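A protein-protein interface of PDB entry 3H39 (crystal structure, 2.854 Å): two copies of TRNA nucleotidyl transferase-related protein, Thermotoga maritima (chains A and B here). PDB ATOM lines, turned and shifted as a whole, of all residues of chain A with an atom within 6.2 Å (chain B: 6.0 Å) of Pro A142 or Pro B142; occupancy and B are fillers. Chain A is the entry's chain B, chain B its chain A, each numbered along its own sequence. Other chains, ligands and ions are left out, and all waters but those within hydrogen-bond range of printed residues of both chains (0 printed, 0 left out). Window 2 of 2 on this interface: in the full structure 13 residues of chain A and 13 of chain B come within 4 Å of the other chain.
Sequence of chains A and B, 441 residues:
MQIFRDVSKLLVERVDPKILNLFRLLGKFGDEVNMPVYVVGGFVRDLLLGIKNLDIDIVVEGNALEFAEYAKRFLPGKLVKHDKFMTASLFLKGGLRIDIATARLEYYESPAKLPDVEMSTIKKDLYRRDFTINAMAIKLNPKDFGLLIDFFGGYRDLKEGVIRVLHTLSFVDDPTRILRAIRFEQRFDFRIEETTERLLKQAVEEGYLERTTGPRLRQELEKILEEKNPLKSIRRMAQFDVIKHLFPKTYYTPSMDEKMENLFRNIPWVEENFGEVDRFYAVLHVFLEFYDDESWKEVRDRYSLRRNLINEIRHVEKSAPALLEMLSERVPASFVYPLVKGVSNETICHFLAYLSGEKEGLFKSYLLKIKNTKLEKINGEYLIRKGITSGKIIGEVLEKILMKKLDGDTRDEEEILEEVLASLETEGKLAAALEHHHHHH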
ATOM      1  N   ARG A  24     -26.634  11.965   5.290  1.00  0.00           N
ATOM      2  CA  ARG A  24     -26.061  13.058   6.083  1.00  0.00           C
ATOM      3  C   ARG A  24     -27.143  13.930   6.710  1.00  0.00           C
ATOM      4  O   ARG A  24     -27.051  14.319   7.877  1.00  0.00           O
ATOM      5  CB  ARG A  24     -25.178  13.954   5.227  1.00  0.00           C
ATOM      6  CG  ARG A  24     -24.127  13.237   4.439  1.00  0.00           C
ATOM      7  CD  ARG A  24     -23.506  14.209   3.472  1.00  0.00           C
ATOM      8  NE  ARG A  24     -22.137  13.848   3.148  1.00  0.00           N
ATOM      9  CZ  ARG A  24     -21.685  13.678   1.915  1.00  0.00           C
ATOM     10  NH1 ARG A  24     -22.498  13.859   0.882  1.00  0.00           N
ATOM     11  NH2 ARG A  24     -20.417  13.348   1.724  1.00  0.00           N
ATOM     12  N   GLY A  27     -28.909  11.866   9.552  1.00  0.00           N
ATOM     13  CA  GLY A  27     -28.084  11.840  10.737  1.00  0.00           C
ATOM     14  C   GLY A  27     -28.149  13.179  11.445  1.00  0.00           C
ATOM     15  O   GLY A  27     -28.322  13.240  12.663  1.00  0.00           O
ATOM     16  N   LYS A  28     -28.011  14.249  10.665  1.00  0.00           N
ATOM     17  CA  LYS A  28     -28.013  15.608  11.193  1.00  0.00           C
ATOM     18  C   LYS A  28     -29.333  15.906  11.941  1.00  0.00           C
ATOM     19  O   LYS A  28     -29.324  16.496  13.019  1.00  0.00           O
ATOM     20  CB  LYS A  28     -27.779  16.607  10.055  1.00  0.00           C
ATOM     21  CG  LYS A  28     -26.895  17.819  10.403  1.00  0.00           C
ATOM     22  CD  LYS A  28     -27.111  18.299  11.808  1.00  0.00           C
ATOM     23  CE  LYS A  28     -26.727  19.737  11.988  1.00  0.00           C
ATOM     24  NZ  LYS A  28     -27.461  20.337  13.142  1.00  0.00           N
ATOM     25  N   ASP A  31     -29.475  14.392  15.451  1.00  0.00           N
ATOM     26  CA  ASP A  31     -28.714  15.188  16.399  1.00  0.00           C
ATOM     27  C   ASP A  31     -29.546  16.373  16.903  1.00  0.00           C
ATOM     28  O   ASP A  31     -29.476  16.752  18.077  1.00  0.00           O
ATOM     29  CB  ASP A  31     -27.425  15.672  15.755  1.00  0.00           C
ATOM     30  CG  ASP A  31     -26.274  14.731  15.993  1.00  0.00           C
ATOM     31  OD1 ASP A  31     -26.537  13.604  16.468  1.00  0.00           O
ATOM     32  OD2 ASP A  31     -25.109  15.118  15.717  1.00  0.00           O
ATOM     33  N   LEU A 140     -25.553   7.265  11.638  1.00  0.00           N
ATOM     34  CA  LEU A 140     -25.627   8.367  10.682  1.00  0.00           C
ATOM     35  C   LEU A 140     -25.385   9.741  11.311  1.00  0.00           C
ATOM     36  O   LEU A 140     -25.008  10.688  10.625  1.00  0.00           O
ATOM     37  CB  LEU A 140     -26.970   8.346   9.960  1.00  0.00           C
ATOM     38  CG  LEU A 140     -27.223   7.161   9.024  1.00  0.00           C
ATOM     39  CD1 LEU A 140     -28.445   7.411   8.134  1.00  0.00           C
ATOM     40  CD2 LEU A 140     -25.985   6.842   8.178  1.00  0.00           C
ATOM     41  N   ASN A 141     -25.593   9.854  12.618  1.00  0.00           N
ATOM     42  CA  ASN A 141     -25.247  11.087  13.299  1.00  0.00           C
ATOM     43  C   ASN A 141     -23.800  11.454  12.958  1.00  0.00           C
ATOM     44  O   ASN A 141     -22.918  10.602  12.959  1.00  0.00           O
ATOM     45  CB  ASN A 141     -25.438  10.951  14.808  1.00  0.00           C
ATOM     46  CG  ASN A 141     -26.745  10.276  15.180  1.00  0.00           C
ATOM     47  OD1 ASN A 141     -27.686  10.930  15.628  1.00  0.00           O
ATOM     48  ND2 ASN A 141     -26.804   8.957  15.014  1.00  0.00           N
ATOM     49  N   PRO A 142     -23.552  12.733  12.676  1.00  0.00           N
ATOM     50  CA  PRO A 142     -22.275  13.240  12.196  1.00  0.00           C
ATOM     51  C   PRO A 142     -21.010  12.807  12.950  1.00  0.00           C
ATOM     52  O   PRO A 142     -19.945  12.771  12.329  1.00  0.00           O
ATOM     53  CB  PRO A 142     -22.469  14.754  12.302  1.00  0.00           C
ATOM     54  CG  PRO A 142     -23.860  14.957  12.069  1.00  0.00           C
ATOM     55  CD  PRO A 142     -24.560  13.803  12.723  1.00  0.00           C
ATOM     56  N   LYS A 143     -21.097  12.534  14.246  1.00  0.00           N
ATOM     57  CA  LYS A 143     -19.900  12.190  15.026  1.00  0.00           C
ATOM     58  C   LYS A 143     -19.423  10.795  14.660  1.00  0.00           C
ATOM     59  O   LYS A 143     -18.232  10.492  14.630  1.00  0.00           O
ATOM     60  CB  LYS A 143     -20.246  12.240  16.503  1.00  0.00           C
ATOM     61  CG  LYS A 143     -19.143  11.854  17.436  1.00  0.00           C
ATOM     62  CD  LYS A 143     -19.581  12.040  18.895  1.00  0.00           C
ATOM     63  CE  LYS A 143     -20.770  11.141  19.282  1.00  0.00           C
ATOM     64  NZ  LYS A 143     -22.094  11.756  18.982  1.00  0.00           N
ATOM     65  N   ASP A 144     -20.369   9.957  14.291  1.00  0.00           N
ATOM     66  CA  ASP A 144     -20.120   8.591  13.931  1.00  0.00           C
ATOM     67  C   ASP A 144     -20.708   8.301  12.593  1.00  0.00           C
ATOM     68  O   ASP A 144     -21.363   7.326  12.440  1.00  0.00           O
ATOM     69  CB  ASP A 144     -20.835   7.690  14.899  1.00  0.00           C
ATOM     70  CG  ASP A 144     -20.416   7.899  16.308  1.00  0.00           C
ATOM     71  OD1 ASP A 144     -21.248   8.269  17.128  1.00  0.00           O
ATOM     72  OD2 ASP A 144     -19.260   7.642  16.626  1.00  0.00           O
ATOM     73  N   PHE A 145     -20.537   9.157  11.616  1.00  0.00           N
ATOM     74  CA  PHE A 145     -21.284   8.937  10.425  1.00  0.00           C
ATOM     75  C   PHE A 145     -21.077   7.665   9.628  1.00  0.00           C
ATOM     76  O   PHE A 145     -22.011   6.918   9.529  1.00  0.00           O
ATOM     77  CB  PHE A 145     -21.143  10.151   9.526  1.00  0.00           C
ATOM     78  CG  PHE A 145     -21.833  10.002   8.236  1.00  0.00           C
ATOM     79  CD1 PHE A 145     -21.139   9.747   7.099  1.00  0.00           C
ATOM     80  CD2 PHE A 145     -23.182  10.080   8.163  1.00  0.00           C
ATOM     81  CE1 PHE A 145     -21.774   9.590   5.944  1.00  0.00           C
ATOM     82  CE2 PHE A 145     -23.800   9.919   6.996  1.00  0.00           C
ATOM     83  CZ  PHE A 145     -23.099   9.674   5.896  1.00  0.00           C
ATOM     84  N   ARG B  24     -26.384  22.552   6.606  1.00  0.00           N
ATOM     85  CA  ARG B  24     -26.115  21.280   7.249  1.00  0.00           C
ATOM     86  C   ARG B  24     -25.110  20.455   6.447  1.00  0.00           C
ATOM     87  O   ARG B  24     -24.279  19.760   7.015  1.00  0.00           O
ATOM     88  CB  ARG B  24     -27.409  20.487   7.413  1.00  0.00           C
ATOM     89  CG  ARG B  24     -28.499  21.195   8.171  1.00  0.00           C
ATOM     90  CD  ARG B  24     -29.718  20.307   8.208  1.00  0.00           C
ATOM     91  NE  ARG B  24     -30.624  20.582   9.315  1.00  0.00           N
ATOM     92  CZ  ARG B  24     -31.861  21.043   9.161  1.00  0.00           C
ATOM     93  NH1 ARG B  24     -32.324  21.286   7.938  1.00  0.00           N
ATOM     94  NH2 ARG B  24     -32.627  21.259  10.230  1.00  0.00           N
ATOM     95  N   GLY B  27     -21.500  22.091   6.343  1.00  0.00           N
ATOM     96  CA  GLY B  27     -20.959  21.746   7.637  1.00  0.00           C
ATOM     97  C   GLY B  27     -20.416  20.331   7.660  1.00  0.00           C
ATOM     98  O   GLY B  27     -19.289  20.120   8.096  1.00  0.00           O
ATOM     99  N   LYS B  28     -21.206  19.358   7.203  1.00  0.00           N
ATOM    100  CA  LYS B  28     -20.734  17.980   7.216  1.00  0.00           C
ATOM    101  C   LYS B  28     -19.554  17.784   6.276  1.00  0.00           C
ATOM    102  O   LYS B  28     -18.601  17.110   6.636  1.00  0.00           O
ATOM    103  CB  LYS B  28     -21.832  16.948   6.928  1.00  0.00           C
ATOM    104  CG  LYS B  28     -21.715  15.756   7.890  1.00  0.00           C
ATOM    105  CD  LYS B  28     -21.847  14.414   7.228  1.00  0.00           C
ATOM    106  CE  LYS B  28     -21.170  13.326   8.062  1.00  0.00           C
ATOM    107  NZ  LYS B  28     -19.705  13.294   7.820  1.00  0.00           N
ATOM    108  N   ASP B  31     -16.523  18.835   7.981  1.00  0.00           N
ATOM    109  CA  ASP B  31     -16.083  17.751   8.869  1.00  0.00           C
ATOM    110  C   ASP B  31     -15.412  16.574   8.144  1.00  0.00           C
ATOM    111  O   ASP B  31     -14.455  15.997   8.637  1.00  0.00           O
ATOM    112  CB  ASP B  31     -17.245  17.255   9.725  1.00  0.00           C
ATOM    113  CG  ASP B  31     -17.415  18.066  10.979  1.00  0.00           C
ATOM    114  OD1 ASP B  31     -16.585  18.969  11.206  1.00  0.00           O
ATOM    115  OD2 ASP B  31     -18.365  17.800  11.746  1.00  0.00           O
ATOM    116  N   LEU B 140     -20.787  26.087  10.915  1.00  0.00           N
ATOM    117  CA  LEU B 140     -21.707  25.142  10.291  1.00  0.00           C
ATOM    118  C   LEU B 140     -21.339  23.670  10.539  1.00  0.00           C
ATOM    119  O   LEU B 140     -22.119  22.761  10.229  1.00  0.00           O
ATOM    120  CB  LEU B 140     -21.777  25.397   8.782  1.00  0.00           C
ATOM    121  CG  LEU B 140     -22.382  26.707   8.276  1.00  0.00           C
ATOM    122  CD1 LEU B 140     -22.680  26.610   6.788  1.00  0.00           C
ATOM    123  CD2 LEU B 140     -23.637  27.090   9.050  1.00  0.00           C
ATOM    124  N   ASN B 141     -20.154  23.419  11.083  1.00  0.00           N
ATOM    125  CA  ASN B 141     -19.782  22.036  11.361  1.00  0.00           C
ATOM    126  C   ASN B 141     -20.765  21.419  12.334  1.00  0.00           C
ATOM    127  O   ASN B 141     -21.176  22.057  13.292  1.00  0.00           O
ATOM    128  CB  ASN B 141     -18.353  21.927  11.874  1.00  0.00           C
ATOM    129  CG  ASN B 141     -17.372  22.607  10.968  1.00  0.00           C
ATOM    130  OD1 ASN B 141     -16.700  21.962  10.180  1.00  0.00           O
ATOM    131  ND2 ASN B 141     -17.304  23.921  11.056  1.00  0.00           N
ATOM    132  N   PRO B 142     -21.163  20.175  12.077  1.00  0.00           N
ATOM    133  CA  PRO B 142     -22.247  19.621  12.882  1.00  0.00           C
ATOM    134  C   PRO B 142     -22.086  19.843  14.390  1.00  0.00           C
ATOM    135  O   PRO B 142     -23.061  20.209  15.074  1.00  0.00           O
ATOM    136  CB  PRO B 142     -22.223  18.149  12.492  1.00  0.00           C
ATOM    137  CG  PRO B 142     -21.854  18.213  11.036  1.00  0.00           C
ATOM    138  CD  PRO B 142     -20.824  19.302  10.940  1.00  0.00           C
ATOM    139  N   LYS B 143     -20.875  19.656  14.901  1.00  0.00           N
ATOM    140  CA  LYS B 143     -20.651  19.781  16.345  1.00  0.00           C
ATOM    141  C   LYS B 143     -21.144  21.112  16.897  1.00  0.00           C
ATOM    142  O   LYS B 143     -21.784  21.141  17.936  1.00  0.00           O
ATOM    143  CB  LYS B 143     -19.179  19.593  16.689  1.00  0.00           C
ATOM    144  CG  LYS B 143     -18.865  19.750  18.158  1.00  0.00           C
ATOM    145  CD  LYS B 143     -17.368  19.927  18.422  1.00  0.00           C
ATOM    146  CE  LYS B 143     -16.682  20.666  17.274  1.00  0.00           C
ATOM    147  NZ  LYS B 143     -15.652  21.624  17.773  1.00  0.00           N
ATOM    148  N   ASP B 144     -20.839  22.207  16.201  1.00  0.00           N
ATOM    149  CA  ASP B 144     -21.174  23.550  16.668  1.00  0.00           C
ATOM    150  C   ASP B 144     -22.143  24.246  15.726  1.00  0.00           C
ATOM    151  O   ASP B 144     -22.020  25.448  15.516  1.00  0.00           O
ATOM    152  CB  ASP B 144     -19.918  24.426  16.737  1.00  0.00           C
ATOM    153  CG  ASP B 144     -18.800  23.810  17.558  1.00  0.00           C
ATOM    154  OD1 ASP B 144     -17.675  23.650  17.023  1.00  0.00           O
ATOM    155  OD2 ASP B 144     -19.046  23.501  18.739  1.00  0.00           O
ATOM    156  N   PHE B 145     -23.108  23.506  15.180  1.00  0.00           N
ATOM    157  CA  PHE B 145     -23.903  23.958  14.031  1.00  0.00           C
ATOM    158  C   PHE B 145     -24.507  25.359  14.106  1.00  0.00           C
ATOM    159  O   PHE B 145     -24.487  26.102  13.127  1.00  0.00           O
ATOM    160  CB  PHE B 145     -24.960  22.935  13.612  1.00  0.00           C
ATOM    161  CG  PHE B 145     -25.856  23.416  12.496  1.00  0.00           C
ATOM    162  CD1 PHE B 145     -27.145  23.829  12.753  1.00  0.00           C
ATOM    163  CD2 PHE B 145     -25.392  23.494  11.198  1.00  0.00           C
ATOM    164  CE1 PHE B 145     -27.937  24.296  11.734  1.00  0.00           C
ATOM    165  CE2 PHE B 145     -26.191  23.949  10.177  1.00  0.00           C
ATOM    166  CZ  PHE B 145     -27.456  24.353  10.436  1.00  0.00           C
ATOM    167  N   GLY B 146     -25.042  25.764  15.235  1.00  0.00           N
ATOM    168  CA  GLY B 146     -25.636  27.091  15.209  1.00  0.00           C
ATOM    169  C   GLY B 146     -24.820  28.246  15.774  1.00  0.00           C
ATOM    170  O   GLY B 146     -25.391  29.279  16.128  1.00  0.00           O
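Of the printed residues of chain B, Lys A28 touches Phe B145. Asp A31 touches none of the printed residues of chain B. Pro A142 touches one residue of chain B. Lys A143 touches none of the printed residues of chain B. Of the printed residues of chain B, Phe A145 touches Lys B28 (3.4 Å). Printed residues of chain A within 4 Å of Lys B28: Arg A24 (3.8 Å) and Phe A145 (3.4 Å). Of the printed residues of chain A, Pro B142 touches Pro A142 (3.4 Å). Of the printed residues of chain A, Phe B145 touches Lys A28. The nearest residue of chain B that does not touch Pro A142 is Lys B28 (4.3 Å). The nearest residue of chain A that does not touch Pro B142 is Lys A28 (4.6 Å). The nearest printed residue of chain A that does not touch Lys B28 is Pro A142 (4.3 Å).
CD of Lys B28 touches CG of Arg A24, at 3.8 Å. Phe B145 touches Lys A28. CB of Pro B142 touches CB of Pro A142, 3.4 Å away. CE of Lys B28 touches CG of Phe A145, 3.4 Å away.
Arg A24 touches Lys B28, but with the chains exchanged Lys A28 does not touch Arg B24 (4.04 Å). Lys A28 touches Phe B145, and with the chains exchanged Phe A145 touches Lys B28. Pro A142 touches its own counterpart, Pro B142. Positions printed for both chains: 24, 27, 28, 31, 140, 141, 142, 143, 144 and 145. Of the 4 pairs that touch across the chains among the printed residues, 3 have their exchanged pair printed and touching as well.
Of the 10 printed residues of chain A, 4 touch a printed residue of chain B. Hydrophobic or aromatic side chains of chain A that line the printed part of chain B: Pro A142 and Phe A145. Among the printed residues, 4 pairs touch across the chains. Among the printed residues, no Asp or Glu carboxylate lies within 4 Å of a Lys or Arg side-chain nitrogen of the other chain.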
